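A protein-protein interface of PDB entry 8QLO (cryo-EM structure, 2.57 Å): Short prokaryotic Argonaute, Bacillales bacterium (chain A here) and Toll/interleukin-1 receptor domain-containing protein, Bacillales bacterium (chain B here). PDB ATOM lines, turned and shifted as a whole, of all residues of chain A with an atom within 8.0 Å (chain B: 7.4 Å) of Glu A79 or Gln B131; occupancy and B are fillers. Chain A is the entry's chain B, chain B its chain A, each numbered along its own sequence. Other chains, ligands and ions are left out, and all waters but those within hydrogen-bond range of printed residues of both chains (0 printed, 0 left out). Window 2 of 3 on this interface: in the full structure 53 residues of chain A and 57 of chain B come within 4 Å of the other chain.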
ATOM      1  N   LEU A  27      -8.862  20.181 -18.467  1.00  0.00           N
ATOM      2  CA  LEU A  27      -7.514  20.077 -19.011  1.00  0.00           C
ATOM      3  C   LEU A  27      -7.054  21.402 -19.602  1.00  0.00           C
ATOM      4  O   LEU A  27      -5.905  21.812 -19.401  1.00  0.00           O
ATOM      5  CB  LEU A  27      -7.451  18.974 -20.065  1.00  0.00           C
ATOM      6  CG  LEU A  27      -7.293  17.535 -19.575  1.00  0.00           C
ATOM      7  CD1 LEU A  27      -7.717  16.561 -20.658  1.00  0.00           C
ATOM      8  CD2 LEU A  27      -5.863  17.275 -19.149  1.00  0.00           C
ATOM      9  N   GLY A  31      -4.995  21.933 -16.425  1.00  0.00           N
ATOM     10  CA  GLY A  31      -4.020  20.934 -16.781  1.00  0.00           C
ATOM     11  C   GLY A  31      -4.289  19.600 -16.119  1.00  0.00           C
ATOM     12  O   GLY A  31      -5.170  19.464 -15.264  1.00  0.00           O
ATOM     13  N   PRO A  32      -3.519  18.588 -16.501  1.00  0.00           N
ATOM     14  CA  PRO A  32      -3.778  17.232 -16.009  1.00  0.00           C
ATOM     15  C   PRO A  32      -3.447  17.082 -14.534  1.00  0.00           C
ATOM     16  O   PRO A  32      -2.700  17.873 -13.956  1.00  0.00           O
ATOM     17  CB  PRO A  32      -2.857  16.372 -16.873  1.00  0.00           C
ATOM     18  CG  PRO A  32      -1.731  17.288 -17.204  1.00  0.00           C
ATOM     19  CD  PRO A  32      -2.359  18.632 -17.403  1.00  0.00           C
ATOM     20  N   ILE A  60      -0.787  20.274 -33.978  1.00  0.00           N
ATOM     21  CA  ILE A  60      -1.576  20.303 -32.752  1.00  0.00           C
ATOM     22  C   ILE A  60      -0.882  21.056 -31.637  1.00  0.00           C
ATOM     23  O   ILE A  60      -1.464  21.215 -30.554  1.00  0.00           O
ATOM     24  CB  ILE A  60      -1.963  18.888 -32.281  1.00  0.00           C
ATOM     25  CG1 ILE A  60      -0.796  18.218 -31.554  1.00  0.00           C
ATOM     26  CG2 ILE A  60      -2.478  18.060 -33.439  1.00  0.00           C
ATOM     27  CD1 ILE A  60      -1.219  17.091 -30.643  1.00  0.00           C
ATOM     28  N   GLN A  61       0.341  21.530 -31.859  1.00  0.00           N
ATOM     29  CA  GLN A  61       0.953  22.511 -30.978  1.00  0.00           C
ATOM     30  C   GLN A  61       0.265  23.860 -31.082  1.00  0.00           C
ATOM     31  O   GLN A  61       0.391  24.691 -30.177  1.00  0.00           O
ATOM     32  CB  GLN A  61       2.442  22.652 -31.300  1.00  0.00           C
ATOM     33  CG  GLN A  61       3.324  21.629 -30.611  1.00  0.00           C
ATOM     34  CD  GLN A  61       3.583  21.968 -29.158  1.00  0.00           C
ATOM     35  OE1 GLN A  61       3.266  23.066 -28.701  1.00  0.00           O
ATOM     36  NE2 GLN A  61       4.158  21.024 -28.424  1.00  0.00           N
ATOM     37  N   LYS A  62      -0.484  24.122 -32.155  1.00  0.00           N
ATOM     38  CA  LYS A  62      -1.125  25.448 -32.390  1.00  0.00           C
ATOM     39  C   LYS A  62      -2.624  25.342 -32.171  1.00  0.00           C
ATOM     40  O   LYS A  62      -3.191  24.369 -32.634  1.00  0.00           O
ATOM     41  CB  LYS A  62      -0.902  25.878 -33.839  1.00  0.00           C
ATOM     42  CG  LYS A  62       0.546  25.863 -34.293  1.00  0.00           C
ATOM     43  CD  LYS A  62       0.675  25.918 -35.787  1.00  0.00           C
ATOM     44  CE  LYS A  62      -0.042  27.113 -36.372  1.00  0.00           C
ATOM     45  NZ  LYS A  62       0.505  28.380 -35.836  1.00  0.00           N
ATOM     46  N   PHE A  75      -9.208  22.834 -28.812  1.00  0.00           N
ATOM     47  CA  PHE A  75      -7.963  22.363 -28.146  1.00  0.00           C
ATOM     48  C   PHE A  75      -6.979  23.531 -28.009  1.00  0.00           C
ATOM     49  O   PHE A  75      -6.404  23.953 -29.032  1.00  0.00           O
ATOM     50  CB  PHE A  75      -7.356  21.192 -28.923  1.00  0.00           C
ATOM     51  CG  PHE A  75      -6.158  20.554 -28.265  1.00  0.00           C
ATOM     52  CD1 PHE A  75      -6.242  20.049 -26.978  1.00  0.00           C
ATOM     53  CD2 PHE A  75      -4.952  20.445 -28.938  1.00  0.00           C
ATOM     54  CE1 PHE A  75      -5.143  19.460 -26.374  1.00  0.00           C
ATOM     55  CE2 PHE A  75      -3.855  19.851 -28.334  1.00  0.00           C
ATOM     56  CZ  PHE A  75      -3.953  19.362 -27.053  1.00  0.00           C
ATOM     57  N   PRO A  76      -6.765  24.077 -26.790  1.00  0.00           N
ATOM     58  CA  PRO A  76      -5.890  25.199 -26.617  1.00  0.00           C
ATOM     59  C   PRO A  76      -4.537  24.895 -27.270  1.00  0.00           C
ATOM     60  O   PRO A  76      -4.125  25.676 -28.043  1.00  0.00           O
ATOM     61  CB  PRO A  76      -5.881  25.333 -25.107  1.00  0.00           C
ATOM     62  CG  PRO A  76      -7.231  24.857 -24.703  1.00  0.00           C
ATOM     63  CD  PRO A  76      -7.424  23.641 -25.573  1.00  0.00           C
ATOM     64  N   GLY A  77      -3.903  23.772 -26.968  1.00  0.00           N
ATOM     65  CA  GLY A  77      -2.609  23.360 -27.551  1.00  0.00           C
ATOM     66  C   GLY A  77      -1.902  22.338 -26.676  1.00  0.00           C
ATOM     67  O   GLY A  77      -2.073  22.422 -25.460  1.00  0.00           O
ATOM     68  N   PHE A  78      -1.081  21.440 -27.238  1.00  0.00           N
ATOM     69  CA  PHE A  78      -0.542  20.401 -26.368  1.00  0.00           C
ATOM     70  C   PHE A  78       0.201  20.998 -25.180  1.00  0.00           C
ATOM     71  O   PHE A  78      -0.073  20.651 -24.026  1.00  0.00           O
ATOM     72  CB  PHE A  78       0.375  19.468 -27.154  1.00  0.00           C
ATOM     73  CG  PHE A  78       0.635  18.168 -26.459  1.00  0.00           C
ATOM     74  CD1 PHE A  78       1.684  18.048 -25.567  1.00  0.00           C
ATOM     75  CD2 PHE A  78      -0.181  17.075 -26.675  1.00  0.00           C
ATOM     76  CE1 PHE A  78       1.921  16.860 -24.914  1.00  0.00           C
ATOM     77  CE2 PHE A  78       0.054  15.884 -26.022  1.00  0.00           C
ATOM     78  CZ  PHE A  78       1.106  15.777 -25.143  1.00  0.00           C
ATOM     79  N   GLU A  79       1.144  21.903 -25.441  1.00  0.00           N
ATOM     80  CA  GLU A  79       1.904  22.496 -24.348  1.00  0.00           C
ATOM     81  C   GLU A  79       1.019  23.374 -23.474  1.00  0.00           C
ATOM     82  O   GLU A  79       1.215  23.444 -22.255  1.00  0.00           O
ATOM     83  CB  GLU A  79       3.080  23.299 -24.898  1.00  0.00           C
ATOM     84  CG  GLU A  79       4.164  23.579 -23.873  1.00  0.00           C
ATOM     85  CD  GLU A  79       5.414  24.159 -24.496  1.00  0.00           C
ATOM     86  OE1 GLU A  79       5.521  24.146 -25.739  1.00  0.00           O
ATOM     87  OE2 GLU A  79       6.293  24.631 -23.744  1.00  0.00           O
ATOM     88  N   ALA A  80       0.042  24.053 -24.078  1.00  0.00           N
ATOM     89  CA  ALA A  80      -0.832  24.934 -23.310  1.00  0.00           C
ATOM     90  C   ALA A  80      -1.717  24.146 -22.354  1.00  0.00           C
ATOM     91  O   ALA A  80      -2.025  24.617 -21.253  1.00  0.00           O
ATOM     92  CB  ALA A  80      -1.682  25.779 -24.256  1.00  0.00           C
ATOM     93  N   VAL A  81      -2.137  22.949 -22.755  1.00  0.00           N
ATOM     94  CA  VAL A  81      -3.050  22.160 -21.934  1.00  0.00           C
ATOM     95  C   VAL A  81      -2.285  21.344 -20.901  1.00  0.00           C
ATOM     96  O   VAL A  81      -2.494  21.486 -19.691  1.00  0.00           O
ATOM     97  CB  VAL A  81      -3.922  21.256 -22.823  1.00  0.00           C
ATOM     98  CG1 VAL A  81      -4.695  20.274 -21.972  1.00  0.00           C
ATOM     99  CG2 VAL A  81      -4.870  22.092 -23.651  1.00  0.00           C
ATOM    100  N   PHE A  82      -1.386  20.478 -21.364  1.00  0.00           N
ATOM    101  CA  PHE A  82      -0.761  19.504 -20.476  1.00  0.00           C
ATOM    102  C   PHE A  82       0.418  20.108 -19.724  1.00  0.00           C
ATOM    103  O   PHE A  82       0.595  19.868 -18.524  1.00  0.00           O
ATOM    104  CB  PHE A  82      -0.332  18.279 -21.281  1.00  0.00           C
ATOM    105  CG  PHE A  82      -1.467  17.605 -21.989  1.00  0.00           C
ATOM    106  CD1 PHE A  82      -2.543  17.103 -21.277  1.00  0.00           C
ATOM    107  CD2 PHE A  82      -1.471  17.489 -23.366  1.00  0.00           C
ATOM    108  CE1 PHE A  82      -3.592  16.489 -21.923  1.00  0.00           C
ATOM    109  CE2 PHE A  82      -2.520  16.877 -24.016  1.00  0.00           C
ATOM    110  CZ  PHE A  82      -3.581  16.376 -23.294  1.00  0.00           C
ATOM    111  N   GLY A  83       1.234  20.892 -20.408  1.00  0.00           N
ATOM    112  CA  GLY A  83       2.429  21.452 -19.831  1.00  0.00           C
ATOM    113  C   GLY A  83       3.713  20.731 -20.184  1.00  0.00           C
ATOM    114  O   GLY A  83       4.758  21.054 -19.607  1.00  0.00           O
ATOM    115  N   CYS A  84       3.668  19.773 -21.103  1.00  0.00           N
ATOM    116  CA  CYS A  84       4.860  19.071 -21.550  1.00  0.00           C
ATOM    117  C   CYS A  84       4.890  19.131 -23.069  1.00  0.00           C
ATOM    118  O   CYS A  84       3.851  19.226 -23.725  1.00  0.00           O
ATOM    119  CB  CYS A  84       4.881  17.624 -21.054  1.00  0.00           C
ATOM    120  SG  CYS A  84       3.418  16.659 -21.489  1.00  0.00           S
ATOM    121  N   LYS A  85       6.094  19.082 -23.622  1.00  0.00           N
ATOM    122  CA  LYS A  85       6.281  19.193 -25.057  1.00  0.00           C
ATOM    123  C   LYS A  85       6.275  17.815 -25.701  1.00  0.00           C
ATOM    124  O   LYS A  85       7.142  16.980 -25.430  1.00  0.00           O
ATOM    125  CB  LYS A  85       7.589  19.913 -25.399  1.00  0.00           C
ATOM    126  CG  LYS A  85       7.534  21.419 -25.220  1.00  0.00           C
ATOM    127  CD  LYS A  85       8.809  22.078 -25.718  1.00  0.00           C
ATOM    128  CE  LYS A  85       8.614  22.705 -27.092  1.00  0.00           C
ATOM    129  NZ  LYS A  85       7.717  21.902 -27.967  1.00  0.00           N
ATOM    130  N   TRP A  86       5.284  17.586 -26.570  1.00  0.00           N
ATOM    131  CA  TRP A  86       5.242  16.330 -27.356  1.00  0.00           C
ATOM    132  C   TRP A  86       5.895  16.653 -28.696  1.00  0.00           C
ATOM    133  O   TRP A  86       5.221  16.525 -29.738  1.00  0.00           O
ATOM    134  CB  TRP A  86       3.785  15.885 -27.537  1.00  0.00           C
ATOM    135  CG  TRP A  86       3.599  14.573 -28.251  1.00  0.00           C
ATOM    136  CD1 TRP A  86       4.567  13.684 -28.611  1.00  0.00           C
ATOM    137  CD2 TRP A  86       2.351  14.019 -28.724  1.00  0.00           C
ATOM    138  NE1 TRP A  86       4.012  12.611 -29.256  1.00  0.00           N
ATOM    139  CE2 TRP A  86       2.656  12.788 -29.343  1.00  0.00           C
ATOM    140  CE3 TRP A  86       1.017  14.436 -28.682  1.00  0.00           C
ATOM    141  CZ2 TRP A  86       1.676  11.980 -29.913  1.00  0.00           C
ATOM    142  CZ3 TRP A  86       0.048  13.635 -29.243  1.00  0.00           C
ATOM    143  CH2 TRP A  86       0.375  12.424 -29.851  1.00  0.00           C
ATOM    144  N   ASP A  87       7.157  17.093 -28.675  1.00  0.00           N
ATOM    145  CA  ASP A  87       7.828  17.546 -29.925  1.00  0.00           C
ATOM    146  C   ASP A  87       7.993  16.386 -30.912  1.00  0.00           C
ATOM    147  O   ASP A  87       8.039  15.225 -30.462  1.00  0.00           O
ATOM    148  CB  ASP A  87       9.174  18.207 -29.618  1.00  0.00           C
ATOM    149  CG  ASP A  87       9.603  19.211 -30.674  1.00  0.00           C
ATOM    150  OD1 ASP A  87       9.704  18.815 -31.851  1.00  0.00           O
ATOM    151  OD2 ASP A  87       9.833  20.380 -30.309  1.00  0.00           O
ATOM    152  N   TRP B  22      -9.373  31.950 -22.699  1.00  0.00           N
ATOM    153  CA  TRP B  22      -8.229  31.101 -22.281  1.00  0.00           C
ATOM    154  C   TRP B  22      -7.166  31.962 -21.603  1.00  0.00           C
ATOM    155  O   TRP B  22      -6.826  31.679 -20.435  1.00  0.00           O
ATOM    156  CB  TRP B  22      -7.638  30.388 -23.504  1.00  0.00           C
ATOM    157  CG  TRP B  22      -6.321  29.710 -23.229  1.00  0.00           C
ATOM    158  CD1 TRP B  22      -6.131  28.501 -22.629  1.00  0.00           C
ATOM    159  CD2 TRP B  22      -5.004  30.231 -23.512  1.00  0.00           C
ATOM    160  NE1 TRP B  22      -4.794  28.220 -22.541  1.00  0.00           N
ATOM    161  CE2 TRP B  22      -4.078  29.264 -23.065  1.00  0.00           C
ATOM    162  CE3 TRP B  22      -4.521  31.406 -24.096  1.00  0.00           C
ATOM    163  CZ2 TRP B  22      -2.702  29.442 -23.187  1.00  0.00           C
ATOM    164  CZ3 TRP B  22      -3.160  31.584 -24.210  1.00  0.00           C
ATOM    165  CH2 TRP B  22      -2.265  30.615 -23.757  1.00  0.00           C
ATOM    166  N   LYS B  26      -6.005  31.822 -17.621  1.00  0.00           N
ATOM    167  CA  LYS B  26      -4.594  31.408 -17.398  1.00  0.00           C
ATOM    168  C   LYS B  26      -3.883  32.493 -16.586  1.00  0.00           C
ATOM    169  O   LYS B  26      -3.284  32.160 -15.538  1.00  0.00           O
ATOM    170  CB  LYS B  26      -3.872  31.195 -18.733  1.00  0.00           C
ATOM    171  CG  LYS B  26      -4.218  29.907 -19.468  1.00  0.00           C
ATOM    172  CD  LYS B  26      -3.913  28.663 -18.666  1.00  0.00           C
ATOM    173  CE  LYS B  26      -4.093  27.388 -19.463  1.00  0.00           C
ATOM    174  NZ  LYS B  26      -3.877  26.183 -18.629  1.00  0.00           N
ATOM    175  N   VAL B 120       4.145  40.336 -28.313  1.00  0.00           N
ATOM    176  CA  VAL B 120       4.327  38.900 -27.933  1.00  0.00           C
ATOM    177  C   VAL B 120       3.590  38.041 -28.964  1.00  0.00           C
ATOM    178  O   VAL B 120       2.455  38.367 -29.273  1.00  0.00           O
ATOM    179  CB  VAL B 120       3.900  38.661 -26.473  1.00  0.00           C
ATOM    180  CG1 VAL B 120       4.576  39.642 -25.532  1.00  0.00           C
ATOM    181  CG2 VAL B 120       2.404  38.720 -26.292  1.00  0.00           C
ATOM    182  N   PHE B 122       1.684  34.774 -30.394  1.00  0.00           N
ATOM    183  CA  PHE B 122       0.954  33.570 -29.951  1.00  0.00           C
ATOM    184  C   PHE B 122       0.487  32.867 -31.214  1.00  0.00           C
ATOM    185  O   PHE B 122      -0.295  31.941 -31.129  1.00  0.00           O
ATOM    186  CB  PHE B 122      -0.260  33.937 -29.105  1.00  0.00           C
ATOM    187  CG  PHE B 122      -0.050  34.355 -27.677  1.00  0.00           C
ATOM    188  CD1 PHE B 122       0.621  35.518 -27.360  1.00  0.00           C
ATOM    189  CD2 PHE B 122      -0.577  33.600 -26.649  1.00  0.00           C
ATOM    190  CE1 PHE B 122       0.781  35.896 -26.040  1.00  0.00           C
ATOM    191  CE2 PHE B 122      -0.413  33.978 -25.329  1.00  0.00           C
ATOM    192  CZ  PHE B 122       0.267  35.127 -25.026  1.00  0.00           C
ATOM    193  N   SER B 125       2.354  29.535 -31.241  1.00  0.00           N
ATOM    194  CA  SER B 125       1.636  28.672 -30.265  1.00  0.00           C
ATOM    195  C   SER B 125       1.206  29.517 -29.061  1.00  0.00           C
ATOM    196  O   SER B 125       1.900  30.508 -28.757  1.00  0.00           O
ATOM    197  CB  SER B 125       2.483  27.501 -29.842  1.00  0.00           C
ATOM    198  OG  SER B 125       1.726  26.588 -29.061  1.00  0.00           O
ATOM    199  N   TRP B 126       0.106  29.138 -28.407  1.00  0.00           N
ATOM    200  CA  TRP B 126      -0.367  29.877 -27.208  1.00  0.00           C
ATOM    201  C   TRP B 126       0.623  29.688 -26.061  1.00  0.00           C
ATOM    202  O   TRP B 126       0.952  30.684 -25.379  1.00  0.00           O
ATOM    203  CB  TRP B 126      -1.766  29.393 -26.809  1.00  0.00           C
ATOM    204  CG  TRP B 126      -2.868  29.940 -27.674  1.00  0.00           C
ATOM    205  CD1 TRP B 126      -2.745  30.799 -28.725  1.00  0.00           C
ATOM    206  CD2 TRP B 126      -4.278  29.654 -27.552  1.00  0.00           C
ATOM    207  NE1 TRP B 126      -3.974  31.069 -29.264  1.00  0.00           N
ATOM    208  CE2 TRP B 126      -4.932  30.383 -28.567  1.00  0.00           C
ATOM    209  CE3 TRP B 126      -5.042  28.861 -26.690  1.00  0.00           C
ATOM    210  CZ2 TRP B 126      -6.313  30.336 -28.740  1.00  0.00           C
ATOM    211  CZ3 TRP B 126      -6.407  28.820 -26.861  1.00  0.00           C
ATOM    212  CH2 TRP B 126      -7.032  29.548 -27.871  1.00  0.00           C
ATOM    213  N   ALA B 127       1.085  28.452 -25.856  1.00  0.00           N
ATOM    214  CA  ALA B 127       2.020  28.163 -24.745  1.00  0.00           C
ATOM    215  C   ALA B 127       3.314  28.962 -24.935  1.00  0.00           C
ATOM    216  O   ALA B 127       3.755  29.603 -23.967  1.00  0.00           O
ATOM    217  CB  ALA B 127       2.298  26.684 -24.684  1.00  0.00           C
ATOM    218  N   VAL B 128       3.892  28.924 -26.139  1.00  0.00           N
ATOM    219  CA  VAL B 128       5.198  29.614 -26.362  1.00  0.00           C
ATOM    220  C   VAL B 128       4.982  31.121 -26.185  1.00  0.00           C
ATOM    221  O   VAL B 128       5.830  31.760 -25.531  1.00  0.00           O
ATOM    222  CB  VAL B 128       5.811  29.255 -27.732  1.00  0.00           C
ATOM    223  CG1 VAL B 128       5.744  27.758 -27.991  1.00  0.00           C
ATOM    224  CG2 VAL B 128       5.176  30.022 -28.882  1.00  0.00           C
ATOM    225  N   GLY B 129       3.871  31.654 -26.706  1.00  0.00           N
ATOM    226  CA  GLY B 129       3.559  33.084 -26.529  1.00  0.00           C
ATOM    227  C   GLY B 129       3.366  33.405 -25.060  1.00  0.00           C
ATOM    228  O   GLY B 129       3.804  34.488 -24.633  1.00  0.00           O
ATOM    229  N   LEU B 130       2.740  32.490 -24.315  1.00  0.00           N
ATOM    230  CA  LEU B 130       2.539  32.690 -22.857  1.00  0.00           C
ATOM    231  C   LEU B 130       3.895  32.957 -22.193  1.00  0.00           C
ATOM    232  O   LEU B 130       4.014  33.990 -21.514  1.00  0.00           O
ATOM    233  CB  LEU B 130       1.869  31.445 -22.269  1.00  0.00           C
ATOM    234  CG  LEU B 130       1.569  31.511 -20.773  1.00  0.00           C
ATOM    235  CD1 LEU B 130       0.369  32.404 -20.503  1.00  0.00           C
ATOM    236  CD2 LEU B 130       1.339  30.119 -20.207  1.00  0.00           C
ATOM    237  N   GLN B 131       4.876  32.065 -22.379  1.00  0.00           N
ATOM    238  CA  GLN B 131       6.157  32.254 -21.704  1.00  0.00           C
ATOM    239  C   GLN B 131       6.740  33.624 -22.014  1.00  0.00           C
ATOM    240  O   GLN B 131       7.192  34.338 -21.111  1.00  0.00           O
ATOM    241  CB  GLN B 131       7.148  31.157 -22.096  1.00  0.00           C
ATOM    242  CG  GLN B 131       6.534  29.809 -22.392  1.00  0.00           C
ATOM    243  CD  GLN B 131       7.542  28.823 -22.949  1.00  0.00           C
ATOM    244  OE1 GLN B 131       8.668  29.191 -23.286  1.00  0.00           O
ATOM    245  NE2 GLN B 131       7.141  27.563 -23.052  1.00  0.00           N
ATOM    246  N   ASP B 132       6.729  33.969 -23.306  1.00  0.00           N
ATOM    247  CA  ASP B 132       7.243  35.293 -23.740  1.00  0.00           C
ATOM    248  C   ASP B 132       6.382  36.381 -23.096  1.00  0.00           C
ATOM    249  O   ASP B 132       6.960  37.334 -22.564  1.00  0.00           O
ATOM    250  CB  ASP B 132       7.250  35.423 -25.264  1.00  0.00           C
ATOM    251  CG  ASP B 132       8.019  34.314 -25.962  1.00  0.00           C
ATOM    252  OD1 ASP B 132       9.214  34.144 -25.647  1.00  0.00           O
ATOM    253  OD2 ASP B 132       7.423  33.642 -26.825  1.00  0.00           O
ATOM    254  N   LEU B 133       5.056  36.226 -23.139  1.00  0.00           N
ATOM    255  CA  LEU B 133       4.150  37.217 -22.498  1.00  0.00           C
ATOM    256  C   LEU B 133       4.497  37.309 -21.009  1.00  0.00           C
ATOM    257  O   LEU B 133       4.723  38.434 -20.526  1.00  0.00           O
ATOM    258  CB  LEU B 133       2.696  36.777 -22.691  1.00  0.00           C
ATOM    259  CG  LEU B 133       1.657  37.642 -21.980  1.00  0.00           C
ATOM    260  CD1 LEU B 133       1.458  38.961 -22.710  1.00  0.00           C
ATOM    261  CD2 LEU B 133       0.335  36.903 -21.843  1.00  0.00           C
ATOM    262  N   LEU B 134       4.569  36.162 -20.327  1.00  0.00           N
ATOM    263  CA  LEU B 134       4.895  36.149 -18.876  1.00  0.00           C
ATOM    264  C   LEU B 134       6.250  36.829 -18.666  1.00  0.00           C
ATOM    265  O   LEU B 134       6.354  37.642 -17.736  1.00  0.00           O
ATOM    266  CB  LEU B 134       4.937  34.702 -18.379  1.00  0.00           C
ATOM    267  CG  LEU B 134       3.579  34.023 -18.213  1.00  0.00           C
ATOM    268  CD1 LEU B 134       3.738  32.667 -17.546  1.00  0.00           C
ATOM    269  CD2 LEU B 134       2.625  34.904 -17.423  1.00  0.00           C
ATOM    270  N   LYS B 135       7.239  36.503 -19.502  1.00  0.00           N
ATOM    271  CA  LYS B 135       8.600  37.074 -19.327  1.00  0.00           C
ATOM    272  C   LYS B 135       8.505  38.600 -19.410  1.00  0.00           C
ATOM    273  O   LYS B 135       9.025  39.270 -18.504  1.00  0.00           O
ATOM    274  CB  LYS B 135       9.545  36.536 -20.404  1.00  0.00           C
ATOM    275  CG  LYS B 135      10.971  37.066 -20.344  1.00  0.00           C
ATOM    276  CD  LYS B 135      11.820  36.613 -21.511  1.00  0.00           C
ATOM    277  CE  LYS B 135      11.834  35.108 -21.682  1.00  0.00           C
ATOM    278  NZ  LYS B 135      12.358  34.425 -20.476  1.00  0.00           N
ATOM    279  N   ALA B 136       7.832  39.114 -20.442  1.00  0.00           N
ATOM    280  CA  ALA B 136       7.704  40.576 -20.631  1.00  0.00           C
ATOM    281  C   ALA B 136       7.017  41.181 -19.404  1.00  0.00           C
ATOM    282  O   ALA B 136       7.512  42.192 -18.904  1.00  0.00           O
ATOM    283  CB  ALA B 136       6.930  40.865 -21.893  1.00  0.00           C
ATOM    284  N   LEU B 137       5.933  40.557 -18.934  1.00  0.00           N
ATOM    285  CA  LEU B 137       5.186  41.083 -17.761  1.00  0.00           C
ATOM    286  C   LEU B 137       6.133  41.173 -16.560  1.00  0.00           C
ATOM    287  O   LEU B 137       6.154  42.228 -15.910  1.00  0.00           O
ATOM    288  CB  LEU B 137       4.006  40.152 -17.466  1.00  0.00           C
ATOM    289  CG  LEU B 137       2.642  40.652 -17.940  1.00  0.00           C
ATOM    290  CD1 LEU B 137       2.602  40.777 -19.455  1.00  0.00           C
ATOM    291  CD2 LEU B 137       1.530  39.734 -17.456  1.00  0.00           C
ATOM    292  N   ASP B 138       6.900  40.113 -16.292  1.00  0.00           N
ATOM    293  CA  ASP B 138       7.813  40.099 -15.119  1.00  0.00           C
ATOM    294  C   ASP B 138       8.874  41.193 -15.284  1.00  0.00           C
ATOM    295  O   ASP B 138       9.174  41.874 -14.288  1.00  0.00           O
ATOM    296  CB  ASP B 138       8.442  38.718 -14.914  1.00  0.00           C
ATOM    297  CG  ASP B 138       7.427  37.639 -14.580  1.00  0.00           C
ATOM    298  OD1 ASP B 138       6.689  37.817 -13.590  1.00  0.00           O
ATOM    299  OD2 ASP B 138       7.393  36.622 -15.299  1.00  0.00           O
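Of the printed residues of chain B, Pro A76 touches Trp B126.
Printed residues of chain B within 4 Å of Ala A80: Trp B22, Lys B26 and Ala B127.
Of the printed residues of chain A, Lys B26 touches Ala A80.
Printed residues of chain A within 4 Å of Ala B127: Glu A79 (3.5 Å) and Ala A80 (3.5 Å).
Phe B122 touches none of the printed residues of chain A.
The nearest residue of chain B that does not touch Glu A79 is Val B128 (4.3 Å).
The nearest residue of chain A that does not touch Gln B131 is Lys A85 (6.3 Å).
The nearest printed residue of chain A that does not touch Trp B126 is Ala A80 (4.4 Å).
Of the 19 printed residues of chain A, 4 touch a printed residue of chain B.
Hydrophobic or aromatic side chains of chain A within 4 Å of the printed part of chain B: Pro A76 and Ala A80.
Of the 18 printed residues of chain B, 6 touch a printed residue of chain A.
Among the printed residues, 7 pairs touch across the chains.
NZ of Lys A85 is in salt-bridge range of OE1 of Glu A79 (3.8 Å).
Among the printed residues, pairs that only touch across the chains: Pro A76 with Trp B126, Glu A79 with Ala B127, Ala A80 with Trp B22, Ala A80 with Lys B26 and Ala A80 with Ala B127.
The backbone carbonyl oxygen (O) of Gln A61 lies within hydrogen-bond range of the side-chain hydroxyl (OG) of Ser B125, 2.6 Å away.
OE2 of Glu A79 lies within hydrogen-bond range of NE2 of Gln B131 (3.1 Å).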
